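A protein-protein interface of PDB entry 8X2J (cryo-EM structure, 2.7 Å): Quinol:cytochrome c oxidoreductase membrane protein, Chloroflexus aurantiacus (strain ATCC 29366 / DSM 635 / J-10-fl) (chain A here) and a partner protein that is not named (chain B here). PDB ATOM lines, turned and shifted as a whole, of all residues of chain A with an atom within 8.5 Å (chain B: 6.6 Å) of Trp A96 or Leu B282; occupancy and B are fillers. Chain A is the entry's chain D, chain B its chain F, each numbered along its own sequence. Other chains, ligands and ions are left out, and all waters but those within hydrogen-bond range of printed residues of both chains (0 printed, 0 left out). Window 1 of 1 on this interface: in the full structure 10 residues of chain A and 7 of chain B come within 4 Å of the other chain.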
ATOM      1  N   PHE A  71      -9.842   7.660  -1.097  1.00  0.00           N
ATOM      2  CA  PHE A  71      -8.951   8.759  -0.737  1.00  0.00           C
ATOM      3  C   PHE A  71      -7.710   8.787  -1.623  1.00  0.00           C
ATOM      4  O   PHE A  71      -7.285   9.864  -2.062  1.00  0.00           O
ATOM      5  CB  PHE A  71      -8.556   8.671   0.733  1.00  0.00           C
ATOM      6  CG  PHE A  71      -8.142   9.989   1.319  1.00  0.00           C
ATOM      7  CD1 PHE A  71      -9.094  10.921   1.702  1.00  0.00           C
ATOM      8  CD2 PHE A  71      -6.801  10.305   1.468  1.00  0.00           C
ATOM      9  CE1 PHE A  71      -8.715  12.137   2.234  1.00  0.00           C
ATOM     10  CE2 PHE A  71      -6.416  11.519   1.997  1.00  0.00           C
ATOM     11  CZ  PHE A  71      -7.374  12.436   2.382  1.00  0.00           C
ATOM     12  N   GLN A  74      -8.368  10.165  -5.332  1.00  0.00           N
ATOM     13  CA  GLN A  74      -8.483  11.621  -5.359  1.00  0.00           C
ATOM     14  C   GLN A  74      -7.153  12.297  -5.063  1.00  0.00           C
ATOM     15  O   GLN A  74      -6.813  13.296  -5.707  1.00  0.00           O
ATOM     16  CB  GLN A  74      -9.525  12.097  -4.353  1.00  0.00           C
ATOM     17  CG  GLN A  74     -10.920  11.614  -4.595  1.00  0.00           C
ATOM     18  CD  GLN A  74     -11.858  12.121  -3.536  1.00  0.00           C
ATOM     19  OE1 GLN A  74     -12.453  13.189  -3.679  1.00  0.00           O
ATOM     20  NE2 GLN A  74     -11.995  11.364  -2.458  1.00  0.00           N
ATOM     21  N   TYR A  75      -6.390  11.757  -4.102  1.00  0.00           N
ATOM     22  CA  TYR A  75      -5.104  12.340  -3.737  1.00  0.00           C
ATOM     23  C   TYR A  75      -4.125  12.291  -4.899  1.00  0.00           C
ATOM     24  O   TYR A  75      -3.567  13.323  -5.287  1.00  0.00           O
ATOM     25  CB  TYR A  75      -4.524  11.614  -2.520  1.00  0.00           C
ATOM     26  CG  TYR A  75      -3.517  12.431  -1.741  1.00  0.00           C
ATOM     27  CD1 TYR A  75      -2.189  12.522  -2.154  1.00  0.00           C
ATOM     28  CD2 TYR A  75      -3.893  13.108  -0.591  1.00  0.00           C
ATOM     29  CE1 TYR A  75      -1.273  13.274  -1.448  1.00  0.00           C
ATOM     30  CE2 TYR A  75      -2.983  13.861   0.119  1.00  0.00           C
ATOM     31  CZ  TYR A  75      -1.675  13.937  -0.311  1.00  0.00           C
ATOM     32  OH  TYR A  75      -0.767  14.685   0.400  1.00  0.00           O
ATOM     33  N   LEU A  79      -3.451  15.687  -6.961  1.00  0.00           N
ATOM     34  CA  LEU A  79      -2.374  16.237  -6.174  1.00  0.00           C
ATOM     35  C   LEU A  79      -1.007  15.744  -6.602  1.00  0.00           C
ATOM     36  O   LEU A  79      -0.019  16.447  -6.360  1.00  0.00           O
ATOM     37  CB  LEU A  79      -2.581  15.873  -4.695  1.00  0.00           C
ATOM     38  CG  LEU A  79      -3.842  16.488  -4.059  1.00  0.00           C
ATOM     39  CD1 LEU A  79      -4.103  16.026  -2.631  1.00  0.00           C
ATOM     40  CD2 LEU A  79      -3.923  17.970  -4.163  1.00  0.00           C
ATOM     41  N   PRO A  90      -6.008  24.011  -1.768  1.00  0.00           N
ATOM     42  CA  PRO A  90      -4.660  23.497  -1.473  1.00  0.00           C
ATOM     43  C   PRO A  90      -4.249  22.315  -2.339  1.00  0.00           C
ATOM     44  O   PRO A  90      -5.068  21.596  -2.915  1.00  0.00           O
ATOM     45  CB  PRO A  90      -4.748  23.083  -0.003  1.00  0.00           C
ATOM     46  CG  PRO A  90      -5.844  23.868   0.548  1.00  0.00           C
ATOM     47  CD  PRO A  90      -6.836  24.010  -0.543  1.00  0.00           C
ATOM     48  N   LEU A  91      -2.931  22.141  -2.435  1.00  0.00           N
ATOM     49  CA  LEU A  91      -2.315  21.061  -3.197  1.00  0.00           C
ATOM     50  C   LEU A  91      -1.638  20.030  -2.294  1.00  0.00           C
ATOM     51  O   LEU A  91      -0.653  19.404  -2.686  1.00  0.00           O
ATOM     52  CB  LEU A  91      -1.319  21.608  -4.215  1.00  0.00           C
ATOM     53  CG  LEU A  91      -1.779  22.005  -5.628  1.00  0.00           C
ATOM     54  CD1 LEU A  91      -2.352  20.803  -6.360  1.00  0.00           C
ATOM     55  CD2 LEU A  91      -2.759  23.163  -5.645  1.00  0.00           C
ATOM     56  N   ASP A  92      -2.163  19.835  -1.090  1.00  0.00           N
ATOM     57  CA  ASP A  92      -1.570  18.921  -0.110  1.00  0.00           C
ATOM     58  C   ASP A  92      -2.691  18.368   0.765  1.00  0.00           C
ATOM     59  O   ASP A  92      -3.863  18.395   0.378  1.00  0.00           O
ATOM     60  CB  ASP A  92      -0.466  19.629   0.695  1.00  0.00           C
ATOM     61  CG  ASP A  92      -0.946  20.901   1.357  1.00  0.00           C
ATOM     62  OD1 ASP A  92      -1.982  21.443   0.927  1.00  0.00           O
ATOM     63  OD2 ASP A  92      -0.280  21.361   2.309  1.00  0.00           O
ATOM     64  N   ILE A  93      -2.327  17.848   1.945  1.00  0.00           N
ATOM     65  CA  ILE A  93      -3.288  17.287   2.896  1.00  0.00           C
ATOM     66  C   ILE A  93      -4.251  18.318   3.477  1.00  0.00           C
ATOM     67  O   ILE A  93      -5.264  17.941   4.077  1.00  0.00           O
ATOM     68  CB  ILE A  93      -2.523  16.551   4.020  1.00  0.00           C
ATOM     69  CG1 ILE A  93      -3.349  15.398   4.606  1.00  0.00           C
ATOM     70  CG2 ILE A  93      -2.086  17.514   5.115  1.00  0.00           C
ATOM     71  CD1 ILE A  93      -3.688  14.313   3.625  1.00  0.00           C
ATOM     72  N   THR A  94      -3.990  19.618   3.288  1.00  0.00           N
ATOM     73  CA  THR A  94      -4.936  20.663   3.667  1.00  0.00           C
ATOM     74  C   THR A  94      -6.195  20.629   2.796  1.00  0.00           C
ATOM     75  O   THR A  94      -7.234  21.175   3.184  1.00  0.00           O
ATOM     76  CB  THR A  94      -4.224  22.018   3.588  1.00  0.00           C
ATOM     77  OG1 THR A  94      -2.933  21.893   4.191  1.00  0.00           O
ATOM     78  CG2 THR A  94      -4.970  23.098   4.362  1.00  0.00           C
ATOM     79  N   ASN A  95      -6.143  19.931   1.656  1.00  0.00           N
ATOM     80  CA  ASN A  95      -7.283  19.694   0.783  1.00  0.00           C
ATOM     81  C   ASN A  95      -8.056  18.437   1.235  1.00  0.00           C
ATOM     82  O   ASN A  95      -8.607  17.690   0.423  1.00  0.00           O
ATOM     83  CB  ASN A  95      -6.761  19.586  -0.661  1.00  0.00           C
ATOM     84  CG  ASN A  95      -7.854  19.588  -1.743  1.00  0.00           C
ATOM     85  OD1 ASN A  95      -7.594  19.522  -2.943  1.00  0.00           O
ATOM     86  ND2 ASN A  95      -9.096  19.690  -1.296  1.00  0.00           N
ATOM     87  N   TRP A  96      -8.016  18.122   2.529  1.00  0.00           N
ATOM     88  CA  TRP A  96      -8.770  16.997   3.072  1.00  0.00           C
ATOM     89  C   TRP A  96     -10.297  17.163   3.056  1.00  0.00           C
ATOM     90  O   TRP A  96     -10.982  16.132   3.022  1.00  0.00           O
ATOM     91  CB  TRP A  96      -8.263  16.644   4.481  1.00  0.00           C
ATOM     92  CG  TRP A  96      -8.763  17.490   5.597  1.00  0.00           C
ATOM     93  CD1 TRP A  96      -8.174  18.609   6.102  1.00  0.00           C
ATOM     94  CD2 TRP A  96      -9.974  17.307   6.334  1.00  0.00           C
ATOM     95  NE1 TRP A  96      -8.938  19.130   7.115  1.00  0.00           N
ATOM     96  CE2 TRP A  96     -10.052  18.349   7.274  1.00  0.00           C
ATOM     97  CE3 TRP A  96     -11.002  16.361   6.289  1.00  0.00           C
ATOM     98  CZ2 TRP A  96     -11.112  18.469   8.160  1.00  0.00           C
ATOM     99  CZ3 TRP A  96     -12.050  16.482   7.166  1.00  0.00           C
ATOM    100  CH2 TRP A  96     -12.096  17.521   8.094  1.00  0.00           C
ATOM    101  N   PRO A  97     -10.907  18.361   3.084  1.00  0.00           N
ATOM    102  CA  PRO A  97     -12.297  18.431   2.631  1.00  0.00           C
ATOM    103  C   PRO A  97     -12.333  18.324   1.119  1.00  0.00           C
ATOM    104  O   PRO A  97     -11.318  18.503   0.445  1.00  0.00           O
ATOM    105  CB  PRO A  97     -12.781  19.802   3.116  1.00  0.00           C
ATOM    106  CG  PRO A  97     -11.861  20.169   4.177  1.00  0.00           C
ATOM    107  CD  PRO A  97     -10.553  19.657   3.706  1.00  0.00           C
ATOM    108  N   ALA A  98     -13.527  18.008   0.603  1.00  0.00           N
ATOM    109  CA  ALA A  98     -13.761  17.632  -0.797  1.00  0.00           C
ATOM    110  C   ALA A  98     -12.953  16.400  -1.201  1.00  0.00           C
ATOM    111  O   ALA A  98     -12.562  16.255  -2.361  1.00  0.00           O
ATOM    112  CB  ALA A  98     -13.504  18.792  -1.769  1.00  0.00           C
ATOM    113  N   MET A  99     -12.690  15.510  -0.242  1.00  0.00           N
ATOM    114  CA  MET A  99     -12.163  14.178  -0.509  1.00  0.00           C
ATOM    115  C   MET A  99     -12.993  13.177   0.285  1.00  0.00           C
ATOM    116  O   MET A  99     -13.112  11.998  -0.080  1.00  0.00           O
ATOM    117  CB  MET A  99     -10.683  14.085  -0.133  1.00  0.00           C
ATOM    118  CG  MET A  99      -9.763  14.925  -1.000  1.00  0.00           C
ATOM    119  SD  MET A  99      -8.021  14.708  -0.603  1.00  0.00           S
ATOM    120  CE  MET A  99      -7.765  13.044  -1.190  1.00  0.00           C
ATOM    121  N   ILE A 100     -13.564  13.687   1.382  1.00  0.00           N
ATOM    122  CA  ILE A 100     -14.439  12.867   2.229  1.00  0.00           C
ATOM    123  C   ILE A 100     -15.676  12.320   1.520  1.00  0.00           C
ATOM    124  O   ILE A 100     -16.007  11.149   1.756  1.00  0.00           O
ATOM    125  CB  ILE A 100     -14.773  13.624   3.522  1.00  0.00           C
ATOM    126  CG1 ILE A 100     -13.497  14.197   4.145  1.00  0.00           C
ATOM    127  CG2 ILE A 100     -15.484  12.736   4.534  1.00  0.00           C
ATOM    128  CD1 ILE A 100     -12.500  13.144   4.580  1.00  0.00           C
ATOM    129  N   PRO A 101     -16.424  13.077   0.675  1.00  0.00           N
ATOM    130  CA  PRO A 101     -17.597  12.449   0.022  1.00  0.00           C
ATOM    131  C   PRO A 101     -17.280  11.279  -0.897  1.00  0.00           C
ATOM    132  O   PRO A 101     -17.911  10.228  -0.771  1.00  0.00           O
ATOM    133  CB  PRO A 101     -18.226  13.619  -0.747  1.00  0.00           C
ATOM    134  CG  PRO A 101     -17.880  14.781   0.034  1.00  0.00           C
ATOM    135  CD  PRO A 101     -16.468  14.537   0.423  1.00  0.00           C
ATOM    136  N   THR A 103     -14.518   9.497  -0.908  1.00  0.00           N
ATOM    137  CA  THR A 103     -13.960   8.476  -0.019  1.00  0.00           C
ATOM    138  C   THR A 103     -15.059   7.647   0.643  1.00  0.00           C
ATOM    139  O   THR A 103     -15.027   6.407   0.624  1.00  0.00           O
ATOM    140  CB  THR A 103     -13.095   9.156   1.046  1.00  0.00           C
ATOM    141  OG1 THR A 103     -11.927   9.717   0.436  1.00  0.00           O
ATOM    142  CG2 THR A 103     -12.676   8.179   2.128  1.00  0.00           C
ATOM    143  N   MET B 277     -23.052  16.732  10.960  1.00  0.00           N
ATOM    144  CA  MET B 277     -23.427  18.138  11.095  1.00  0.00           C
ATOM    145  C   MET B 277     -22.217  19.050  11.242  1.00  0.00           C
ATOM    146  O   MET B 277     -22.308  20.235  10.904  1.00  0.00           O
ATOM    147  CB  MET B 277     -24.365  18.344  12.286  1.00  0.00           C
ATOM    148  CG  MET B 277     -25.599  17.469  12.272  1.00  0.00           C
ATOM    149  SD  MET B 277     -26.756  17.853  10.956  1.00  0.00           S
ATOM    150  CE  MET B 277     -27.784  19.050  11.774  1.00  0.00           C
ATOM    151  N   SER B 278     -21.094  18.537  11.747  1.00  0.00           N
ATOM    152  CA  SER B 278     -19.869  19.332  11.762  1.00  0.00           C
ATOM    153  C   SER B 278     -19.234  19.409  10.374  1.00  0.00           C
ATOM    154  O   SER B 278     -18.844  20.495   9.920  1.00  0.00           O
ATOM    155  CB  SER B 278     -18.885  18.754  12.781  1.00  0.00           C
ATOM    156  OG  SER B 278     -18.277  17.575  12.294  1.00  0.00           O
ATOM    157  N   TYR B 279     -19.146  18.268   9.674  1.00  0.00           N
ATOM    158  CA  TYR B 279     -18.479  18.238   8.379  1.00  0.00           C
ATOM    159  C   TYR B 279     -19.273  18.964   7.305  1.00  0.00           C
ATOM    160  O   TYR B 279     -18.670  19.550   6.403  1.00  0.00           O
ATOM    161  CB  TYR B 279     -18.214  16.800   7.932  1.00  0.00           C
ATOM    162  CG  TYR B 279     -17.584  16.744   6.560  1.00  0.00           C
ATOM    163  CD1 TYR B 279     -16.319  17.275   6.342  1.00  0.00           C
ATOM    164  CD2 TYR B 279     -18.278  16.227   5.470  1.00  0.00           C
ATOM    165  CE1 TYR B 279     -15.743  17.257   5.092  1.00  0.00           C
ATOM    166  CE2 TYR B 279     -17.707  16.205   4.211  1.00  0.00           C
ATOM    167  CZ  TYR B 279     -16.441  16.723   4.032  1.00  0.00           C
ATOM    168  OH  TYR B 279     -15.860  16.712   2.789  1.00  0.00           O
ATOM    169  N   GLY B 280     -20.608  18.937   7.374  1.00  0.00           N
ATOM    170  CA  GLY B 280     -21.405  19.652   6.388  1.00  0.00           C
ATOM    171  C   GLY B 280     -21.193  21.151   6.448  1.00  0.00           C
ATOM    172  O   GLY B 280     -20.962  21.794   5.421  1.00  0.00           O
ATOM    173  N   GLN B 281     -21.201  21.708   7.662  1.00  0.00           N
ATOM    174  CA  GLN B 281     -20.894  23.119   7.870  1.00  0.00           C
ATOM    175  C   GLN B 281     -19.471  23.452   7.446  1.00  0.00           C
ATOM    176  O   GLN B 281     -19.238  24.480   6.793  1.00  0.00           O
ATOM    177  CB  GLN B 281     -21.106  23.473   9.338  1.00  0.00           C
ATOM    178  CG  GLN B 281     -20.648  24.854   9.739  1.00  0.00           C
ATOM    179  CD  GLN B 281     -20.592  25.026  11.238  1.00  0.00           C
ATOM    180  OE1 GLN B 281     -21.023  24.155  11.991  1.00  0.00           O
ATOM    181  NE2 GLN B 281     -20.053  26.148  11.681  1.00  0.00           N
ATOM    182  N   LEU B 282     -18.519  22.574   7.781  1.00  0.00           N
ATOM    183  CA  LEU B 282     -17.123  22.812   7.429  1.00  0.00           C
ATOM    184  C   LEU B 282     -16.915  22.811   5.919  1.00  0.00           C
ATOM    185  O   LEU B 282     -16.250  23.700   5.384  1.00  0.00           O
ATOM    186  CB  LEU B 282     -16.233  21.764   8.092  1.00  0.00           C
ATOM    187  CG  LEU B 282     -14.834  21.588   7.508  1.00  0.00           C
ATOM    188  CD1 LEU B 282     -13.940  22.778   7.810  1.00  0.00           C
ATOM    189  CD2 LEU B 282     -14.247  20.335   8.062  1.00  0.00           C
ATOM    190  N   VAL B 283     -17.496  21.838   5.212  1.00  0.00           N
ATOM    191  CA  VAL B 283     -17.284  21.760   3.771  1.00  0.00           C
ATOM    192  C   VAL B 283     -18.051  22.862   3.048  1.00  0.00           C
ATOM    193  O   VAL B 283     -17.576  23.371   2.028  1.00  0.00           O
ATOM    194  CB  VAL B 283     -17.613  20.345   3.235  1.00  0.00           C
ATOM    195  CG1 VAL B 283     -19.105  20.058   3.193  1.00  0.00           C
ATOM    196  CG2 VAL B 283     -16.996  20.131   1.858  1.00  0.00           C
ATOM    197  N   ILE B 284     -19.190  23.312   3.592  1.00  0.00           N
ATOM    198  CA  ILE B 284     -19.933  24.403   2.966  1.00  0.00           C
ATOM    199  C   ILE B 284     -19.164  25.714   3.092  1.00  0.00           C
ATOM    200  O   ILE B 284     -18.972  26.433   2.104  1.00  0.00           O
ATOM    201  CB  ILE B 284     -21.347  24.495   3.567  1.00  0.00           C
ATOM    202  CG1 ILE B 284     -22.243  23.462   2.897  1.00  0.00           C
ATOM    203  CG2 ILE B 284     -21.952  25.872   3.376  1.00  0.00           C
ATOM    204  CD1 ILE B 284     -23.452  23.056   3.681  1.00  0.00           C
ATOM    205  N   ILE B 285     -18.665  26.012   4.295  1.00  0.00           N
ATOM    206  CA  ILE B 285     -17.905  27.240   4.505  1.00  0.00           C
ATOM    207  C   ILE B 285     -16.543  27.178   3.809  1.00  0.00           C
ATOM    208  O   ILE B 285     -16.069  28.183   3.266  1.00  0.00           O
ATOM    209  CB  ILE B 285     -17.809  27.505   6.021  1.00  0.00           C
ATOM    210  CG1 ILE B 285     -19.208  27.804   6.570  1.00  0.00           C
ATOM    211  CG2 ILE B 285     -16.863  28.650   6.348  1.00  0.00           C
ATOM    212  CD1 ILE B 285     -19.270  28.006   8.063  1.00  0.00           C
ATOM    213  N   TRP B 286     -15.918  25.999   3.761  1.00  0.00           N
ATOM    214  CA  TRP B 286     -14.609  25.853   3.135  1.00  0.00           C
ATOM    215  C   TRP B 286     -14.698  25.958   1.617  1.00  0.00           C
ATOM    216  O   TRP B 286     -13.879  26.641   0.992  1.00  0.00           O
ATOM    217  CB  TRP B 286     -14.002  24.513   3.559  1.00  0.00           C
ATOM    218  CG  TRP B 286     -12.627  24.213   3.035  1.00  0.00           C
ATOM    219  CD1 TRP B 286     -11.442  24.616   3.571  1.00  0.00           C
ATOM    220  CD2 TRP B 286     -12.299  23.415   1.891  1.00  0.00           C
ATOM    221  NE1 TRP B 286     -10.397  24.132   2.826  1.00  0.00           N
ATOM    222  CE2 TRP B 286     -10.897  23.392   1.786  1.00  0.00           C
ATOM    223  CE3 TRP B 286     -13.057  22.728   0.940  1.00  0.00           C
ATOM    224  CZ2 TRP B 286     -10.237  22.707   0.772  1.00  0.00           C
ATOM    225  CZ3 TRP B 286     -12.398  22.050  -0.066  1.00  0.00           C
ATOM    226  CH2 TRP B 286     -11.003  22.045  -0.143  1.00  0.00           C
ATOM    227  N   SER B 287     -15.680  25.291   1.003  1.00  0.00           N
ATOM    228  CA  SER B 287     -15.816  25.318  -0.445  1.00  0.00           C
ATOM    229  C   SER B 287     -16.385  26.643  -0.935  1.00  0.00           C
ATOM    230  O   SER B 287     -15.921  27.179  -1.946  1.00  0.00           O
ATOM    231  CB  SER B 287     -16.694  24.158  -0.901  1.00  0.00           C
ATOM    232  OG  SER B 287     -16.267  22.938  -0.326  1.00  0.00           O
ATOM    233  N   TYR B 297     -13.786  29.493  10.967  1.00  0.00           N
ATOM    234  CA  TYR B 297     -12.798  28.430  10.888  1.00  0.00           C
ATOM    235  C   TYR B 297     -11.370  28.953  10.925  1.00  0.00           C
ATOM    236  O   TYR B 297     -10.459  28.197  11.281  1.00  0.00           O
ATOM    237  CB  TYR B 297     -13.050  27.591   9.638  1.00  0.00           C
ATOM    238  CG  TYR B 297     -14.169  26.606   9.863  1.00  0.00           C
ATOM    239  CD1 TYR B 297     -13.963  25.462  10.620  1.00  0.00           C
ATOM    240  CD2 TYR B 297     -15.446  26.849   9.370  1.00  0.00           C
ATOM    241  CE1 TYR B 297     -14.987  24.569  10.852  1.00  0.00           C
ATOM    242  CE2 TYR B 297     -16.480  25.960   9.597  1.00  0.00           C
ATOM    243  CZ  TYR B 297     -16.242  24.822  10.339  1.00  0.00           C
ATOM    244  OH  TYR B 297     -17.258  23.928  10.575  1.00  0.00           O
ATOM    245  N   LEU B 310      -8.042  18.554  15.006  1.00  0.00           N
ATOM    246  CA  LEU B 310      -7.533  17.236  14.638  1.00  0.00           C
ATOM    247  C   LEU B 310      -7.818  16.198  15.719  1.00  0.00           C
ATOM    248  O   LEU B 310      -8.074  15.032  15.403  1.00  0.00           O
ATOM    249  CB  LEU B 310      -6.034  17.316  14.356  1.00  0.00           C
ATOM    250  CG  LEU B 310      -5.619  17.954  13.029  1.00  0.00           C
ATOM    251  CD1 LEU B 310      -4.162  18.377  13.077  1.00  0.00           C
ATOM    252  CD2 LEU B 310      -5.861  17.001  11.874  1.00  0.00           C
ATOM    253  N   MET B 313     -11.284  15.238  15.140  1.00  0.00           N
ATOM    254  CA  MET B 313     -11.353  14.293  14.030  1.00  0.00           C
ATOM    255  C   MET B 313     -10.936  12.892  14.464  1.00  0.00           C
ATOM    256  O   MET B 313     -11.545  11.902  14.045  1.00  0.00           O
ATOM    257  CB  MET B 313     -10.472  14.765  12.873  1.00  0.00           C
ATOM    258  CG  MET B 313     -10.999  15.970  12.120  1.00  0.00           C
ATOM    259  SD  MET B 313      -9.823  16.520  10.872  1.00  0.00           S
ATOM    260  CE  MET B 313      -9.492  18.188  11.428  1.00  0.00           C
ATOM    261  N   TRP B 353     -13.763  23.606  21.717  1.00  0.00           N
ATOM    262  CA  TRP B 353     -13.382  24.064  20.385  1.00  0.00           C
ATOM    263  C   TRP B 353     -14.447  24.956  19.757  1.00  0.00           C
ATOM    264  O   TRP B 353     -14.131  25.779  18.893  1.00  0.00           O
ATOM    265  CB  TRP B 353     -13.115  22.854  19.495  1.00  0.00           C
ATOM    266  CG  TRP B 353     -12.557  23.166  18.149  1.00  0.00           C
ATOM    267  CD1 TRP B 353     -11.300  23.608  17.864  1.00  0.00           C
ATOM    268  CD2 TRP B 353     -13.228  23.028  16.894  1.00  0.00           C
ATOM    269  NE1 TRP B 353     -11.150  23.765  16.509  1.00  0.00           N
ATOM    270  CE2 TRP B 353     -12.320  23.414  15.890  1.00  0.00           C
ATOM    271  CE3 TRP B 353     -14.512  22.619  16.520  1.00  0.00           C
ATOM    272  CZ2 TRP B 353     -12.655  23.404  14.539  1.00  0.00           C
ATOM    273  CZ3 TRP B 353     -14.842  22.612  15.180  1.00  0.00           C
ATOM    274  CH2 TRP B 353     -13.917  23.001  14.205  1.00  0.00           C
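N of Ala A98 lies within hydrogen-bond range of OH of Tyr B279 (3.4 Å).
ND2 of Asn A95 sits at hydrogen-bond distance from O of Pro A97 (3.1 Å).
The backbone carbonyl oxygen of Pro A90 sits close to the side-chain amide oxygen of Asn A95 (3.3 Å).
The backbone carbonyl oxygen (O) of Ala A98 lies close to the side-chain amide oxygen (OE1) of Gln A74, 3.3 Å away.
N of Leu B282 lies close to OH of Tyr B297 (3.4 Å).
Pro A90 touches Trp B286 (CD to CZ2, 3.9 Å).
Trp B286 touches Asn A95.
CH2 of Trp A96 touches CD2 of Leu B282, at 3.5 Å.
Met B313 touches Trp A96.
Tyr B279 touches Pro A97.
Pro A97 touches Trp B286 (O to CH2, 3.6 Å).
CZ3 of Trp B286 touches CB of Ala A98 (3.8 Å).
Ile A100 touches Tyr B279.
Tyr B279 touches Pro A101 (OH to CD, 3.3 Å).
Of chain B, only Leu B282 (3.5 Å) and Met B313 (3.6 Å) come within 4 Å of Trp A96.
Leu B282 touches just one residue of chain A: Trp A96.
Of the printed residues of chain A, Met B313 touches Trp A96.
Printed residues of chain B within 4 Å of Pro A90: Trp B286.
Of the printed residues of chain B, Ile A100 touches Tyr B279 (3.4 Å).
Printed residues of chain A within 4 Å of Trp B286: Pro A90 (3.9 Å), Asn A95 (3.2 Å), Pro A97 (3.6 Å) and Ala A98 (3.8 Å).
Tyr A75 touches none of the printed residues of chain B.
Val B283 touches none of the printed residues of chain A.
The nearest residue of chain B that does not touch Trp A96 is Tyr B279 (4.3 Å).
The nearest printed residue of chain B that does not touch Pro A90 is Ser B287 (9.1 Å).
Of the 15 printed residues of chain B, 4 touch a printed residue of chain A.
Hydrophobic or aromatic side chains of chain B within 4 Å of the printed part of chain A: Tyr B279, Leu B282, Trp B286 and Met B313.
Of the 17 printed residues of chain A, 7 touch a printed residue of chain B.
Hydrophobic or aromatic side chains of chain A within 4 Å of the printed part of chain B: Pro A90, Trp A96, Pro A97, Ala A98, Ile A100 and Pro A101.
Among the printed residues, 10 pairs touch across the chains.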
